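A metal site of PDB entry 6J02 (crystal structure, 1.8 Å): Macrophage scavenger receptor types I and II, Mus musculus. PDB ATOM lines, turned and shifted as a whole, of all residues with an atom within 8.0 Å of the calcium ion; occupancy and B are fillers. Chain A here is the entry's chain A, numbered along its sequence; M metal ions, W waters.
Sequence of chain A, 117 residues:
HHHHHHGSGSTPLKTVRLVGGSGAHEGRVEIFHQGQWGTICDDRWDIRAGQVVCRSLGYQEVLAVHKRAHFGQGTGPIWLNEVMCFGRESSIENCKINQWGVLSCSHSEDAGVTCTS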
ATOM      1  N   CYS A  41     -20.715   4.216  -6.675  1.00  0.00           N
ATOM      2  CA  CYS A  41     -21.173   4.630  -5.366  1.00  0.00           C
ATOM      3  C   CYS A  41     -19.994   4.671  -4.397  1.00  0.00           C
ATOM      4  O   CYS A  41     -19.022   3.900  -4.515  1.00  0.00           O
ATOM      5  CB  CYS A  41     -22.246   3.689  -4.831  1.00  0.00           C
ATOM      6  SG  CYS A  41     -22.964   4.151  -3.244  1.00  0.00           S
ATOM      7  N   ASP A  42     -20.097   5.551  -3.409  1.00  0.00           N
ATOM      8  CA  ASP A  42     -18.981   5.741  -2.482  1.00  0.00           C
ATOM      9  C   ASP A  42     -18.983   4.766  -1.293  1.00  0.00           C
ATOM     10  O   ASP A  42     -18.079   4.847  -0.455  1.00  0.00           O
ATOM     11  CB  ASP A  42     -18.968   7.174  -1.953  1.00  0.00           C
ATOM     12  CG  ASP A  42     -20.179   7.499  -1.081  1.00  0.00           C
ATOM     13  OD1 ASP A  42     -20.888   6.558  -0.651  1.00  0.00           O
ATOM     14  OD2 ASP A  42     -20.373   8.701  -0.808  1.00  0.00           O
ATOM     15  N   ASP A  43     -19.964   3.875  -1.204  1.00  0.00           N
ATOM     16  CA  ASP A  43     -20.145   3.082   0.022  1.00  0.00           C
ATOM     17  C   ASP A  43     -18.896   2.289   0.347  1.00  0.00           C
ATOM     18  O   ASP A  43     -18.425   2.286   1.495  1.00  0.00           O
ATOM     19  CB  ASP A  43     -21.340   2.131  -0.136  1.00  0.00           C
ATOM     20  CG  ASP A  43     -22.637   2.808   0.133  1.00  0.00           C
ATOM     21  OD1 ASP A  43     -22.593   3.977   0.538  1.00  0.00           O
ATOM     22  OD2 ASP A  43     -23.709   2.174  -0.016  1.00  0.00           O
ATOM     23  N   ARG A  44     -18.326   1.614  -0.644  1.00  0.00           N
ATOM     24  CA  ARG A  44     -17.159   0.770  -0.453  1.00  0.00           C
ATOM     25  C   ARG A  44     -15.916   1.355  -1.116  1.00  0.00           C
ATOM     26  O   ARG A  44     -14.926   0.649  -1.291  1.00  0.00           O
ATOM     27  CB  ARG A  44     -17.426  -0.631  -0.984  1.00  0.00           C
ATOM     28  CG  ARG A  44     -18.494  -1.352  -0.216  1.00  0.00           C
ATOM     29  CD  ARG A  44     -19.372  -2.138  -1.142  1.00  0.00           C
ATOM     30  NE  ARG A  44     -20.435  -2.865  -0.445  1.00  0.00           N
ATOM     31  CZ  ARG A  44     -21.657  -2.382  -0.215  1.00  0.00           C
ATOM     32  NH1 ARG A  44     -21.996  -1.169  -0.585  1.00  0.00           N
ATOM     33  NH2 ARG A  44     -22.542  -3.137   0.413  1.00  0.00           N
ATOM     34  N   TRP A  45     -15.960   2.641  -1.447  1.00  0.00           N
ATOM     35  CA  TRP A  45     -14.916   3.244  -2.251  1.00  0.00           C
ATOM     36  C   TRP A  45     -13.660   3.445  -1.402  1.00  0.00           C
ATOM     37  O   TRP A  45     -13.711   4.127  -0.384  1.00  0.00           O
ATOM     38  CB  TRP A  45     -15.417   4.570  -2.797  1.00  0.00           C
ATOM     39  CG  TRP A  45     -14.525   5.215  -3.792  1.00  0.00           C
ATOM     40  CD1 TRP A  45     -13.963   6.449  -3.697  1.00  0.00           C
ATOM     41  CD2 TRP A  45     -14.115   4.679  -5.057  1.00  0.00           C
ATOM     42  NE1 TRP A  45     -13.216   6.709  -4.824  1.00  0.00           N
ATOM     43  CE2 TRP A  45     -13.291   5.648  -5.674  1.00  0.00           C
ATOM     44  CE3 TRP A  45     -14.382   3.493  -5.736  1.00  0.00           C
ATOM     45  CZ2 TRP A  45     -12.715   5.436  -6.940  1.00  0.00           C
ATOM     46  CZ3 TRP A  45     -13.820   3.285  -6.972  1.00  0.00           C
ATOM     47  CH2 TRP A  45     -12.987   4.255  -7.559  1.00  0.00           C
ATOM     48  N   LYS A  67     -15.544  10.926  -1.462  1.00  0.00           N
ATOM     49  CA  LYS A  67     -16.911  10.422  -1.338  1.00  0.00           C
ATOM     50  C   LYS A  67     -17.896  11.573  -1.499  1.00  0.00           C
ATOM     51  O   LYS A  67     -17.515  12.738  -1.611  1.00  0.00           O
ATOM     52  CB  LYS A  67     -17.089   9.712   0.003  1.00  0.00           C
ATOM     53  CG  LYS A  67     -15.930   8.749   0.327  1.00  0.00           C
ATOM     54  CD  LYS A  67     -16.232   7.787   1.473  1.00  0.00           C
ATOM     55  CE  LYS A  67     -15.073   6.787   1.665  1.00  0.00           C
ATOM     56  NZ  LYS A  67     -15.221   5.944   2.859  1.00  0.00           N
ATOM     57  N   ARG A  68     -19.182  11.222  -1.546  1.00  0.00           N
ATOM     58  CA  ARG A  68     -20.282  12.189  -1.429  1.00  0.00           C
ATOM     59  C   ARG A  68     -20.268  13.231  -2.544  1.00  0.00           C
ATOM     60  O   ARG A  68     -20.489  14.423  -2.312  1.00  0.00           O
ATOM     61  CB  ARG A  68     -20.288  12.862  -0.050  1.00  0.00           C
ATOM     62  CG  ARG A  68     -20.743  11.955   1.066  1.00  0.00           C
ATOM     63  CD  ARG A  68     -20.614  12.623   2.407  1.00  0.00           C
ATOM     64  NE  ARG A  68     -19.209  12.826   2.747  1.00  0.00           N
ATOM     65  CZ  ARG A  68     -18.409  11.894   3.268  1.00  0.00           C
ATOM     66  NH1 ARG A  68     -18.858  10.670   3.526  1.00  0.00           N
ATOM     67  NH2 ARG A  68     -17.142  12.193   3.542  1.00  0.00           N
ATOM     68  N   ASN A  81     -21.047  -0.543  -6.998  1.00  0.00           N
ATOM     69  CA  ASN A  81     -21.038  -0.259  -5.580  1.00  0.00           C
ATOM     70  C   ASN A  81     -20.244  -1.365  -4.908  1.00  0.00           C
ATOM     71  O   ASN A  81     -19.267  -1.114  -4.200  1.00  0.00           O
ATOM     72  CB  ASN A  81     -22.459  -0.175  -5.004  1.00  0.00           C
ATOM     73  CG  ASN A  81     -22.463   0.367  -3.592  1.00  0.00           C
ATOM     74  OD1 ASN A  81     -21.420   0.731  -3.058  1.00  0.00           O
ATOM     75  ND2 ASN A  81     -23.638   0.459  -2.992  1.00  0.00           N
ATOM     76  N   SER A 104     -29.264   0.869  -4.640  1.00  0.00           N
ATOM     77  CA  SER A 104     -29.121   1.147  -3.220  1.00  0.00           C
ATOM     78  C   SER A 104     -28.397   2.444  -2.950  1.00  0.00           C
ATOM     79  O   SER A 104     -28.111   2.742  -1.788  1.00  0.00           O
ATOM     80  CB  SER A 104     -28.347   0.011  -2.560  1.00  0.00           C
ATOM     81  OG  SER A 104     -27.089  -0.119  -3.201  1.00  0.00           O
ATOM     82  N   CYS A 105     -28.058   3.209  -3.985  1.00  0.00           N
ATOM     83  CA  CYS A 105     -27.330   4.458  -3.827  1.00  0.00           C
ATOM     84  C   CYS A 105     -28.035   5.523  -4.641  1.00  0.00           C
ATOM     85  O   CYS A 105     -28.900   5.251  -5.468  1.00  0.00           O
ATOM     86  CB  CYS A 105     -25.865   4.367  -4.303  1.00  0.00           C
ATOM     87  SG  CYS A 105     -24.847   3.248  -3.378  1.00  0.00           S
ATOM     88  N   SER A 106     -27.622   6.762  -4.407  1.00  0.00           N
ATOM     89  CA  SER A 106     -28.037   7.866  -5.245  1.00  0.00           C
ATOM     90  C   SER A 106     -26.827   8.635  -5.707  1.00  0.00           C
ATOM     91  O   SER A 106     -25.716   8.492  -5.169  1.00  0.00           O
ATOM     92  CB  SER A 106     -29.016   8.801  -4.506  1.00  0.00           C
ATOM     93  OG  SER A 106     -28.355   9.476  -3.469  1.00  0.00           O
ATOM     94  N   SER A 108     -25.858  11.455  -5.150  1.00  0.00           N
ATOM     95  CA  SER A 108     -25.195  12.251  -4.126  1.00  0.00           C
ATOM     96  C   SER A 108     -24.013  11.514  -3.519  1.00  0.00           C
ATOM     97  O   SER A 108     -23.186  12.136  -2.823  1.00  0.00           O
ATOM     98  CB  SER A 108     -26.190  12.615  -3.018  1.00  0.00           C
ATOM     99  OG  SER A 108     -26.604  11.472  -2.305  1.00  0.00           O
ATOM    100  N   GLU A 109     -23.896  10.213  -3.789  1.00  0.00           N
ATOM    101  CA  GLU A 109     -22.841   9.371  -3.279  1.00  0.00           C
ATOM    102  C   GLU A 109     -21.775   9.067  -4.323  1.00  0.00           C
ATOM    103  O   GLU A 109     -20.957   8.169  -4.110  1.00  0.00           O
ATOM    104  CB  GLU A 109     -23.445   8.057  -2.778  1.00  0.00           C
ATOM    105  CG  GLU A 109     -24.492   8.214  -1.682  1.00  0.00           C
ATOM    106  CD  GLU A 109     -25.045   6.915  -1.269  1.00  0.00           C
ATOM    107  OE1 GLU A 109     -26.114   6.505  -1.757  1.00  0.00           O
ATOM    108  OE2 GLU A 109     -24.367   6.266  -0.474  1.00  0.00           O
ATOM    109  N   ASP A 110     -21.741   9.813  -5.443  1.00  0.00           N
ATOM    110  CA  ASP A 110     -20.864   9.419  -6.535  1.00  0.00           C
ATOM    111  C   ASP A 110     -19.408   9.597  -6.114  1.00  0.00           C
ATOM    112  O   ASP A 110     -19.034  10.652  -5.591  1.00  0.00           O
ATOM    113  CB  ASP A 110     -21.147  10.230  -7.796  1.00  0.00           C
ATOM    114  CG  ASP A 110     -22.392   9.745  -8.551  1.00  0.00           C
ATOM    115  OD1 ASP A 110     -22.898   8.627  -8.278  1.00  0.00           O
ATOM    116  OD2 ASP A 110     -22.845  10.487  -9.448  1.00  0.00           O
HETATM  117 CA    CA M   1     -22.569   6.253   0.882  1.00  0.00          CA
HETATM  118  O   HOH W   1     -20.985   6.055   2.556  1.00  0.00           O
HETATM  119  O   HOH W   2     -22.187   8.762   1.224  1.00  0.00           O
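N of Ser 106 lies within hydrogen-bond range of OE1 of Glu 109 (3.1 Å).
The backbone NH of Arg 68 lies within hydrogen-bond range of the side-chain carboxylate of Asp 42, at 2.9 Å.
The backbone NH (N) of Asp 43 lies close to the side-chain sulfur (SG) of Cys 41.
NH1 of Arg 44 is in salt-bridge range of OD2 of Asp 43, 3.8 Å away.
OD2 of Asp 43 is in hydrogen-bond range of ND2 of Asn 81 (3.4 Å).
SG of Cys 41 is disulfide-bonded to SG of Cys 105 (2.1 Å).
The nearest printed residue that does not touch the calcium ion is Cys 41 (4.6 Å).
The calcium ion is bound by OE2 of Glu 109 (2.3 Å), OD1 of Asp 42 (2.3 Å), OD1 of Asp 43 (2.3 Å), water W1 (2.3 Å) and water W2 (2.6 Å).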
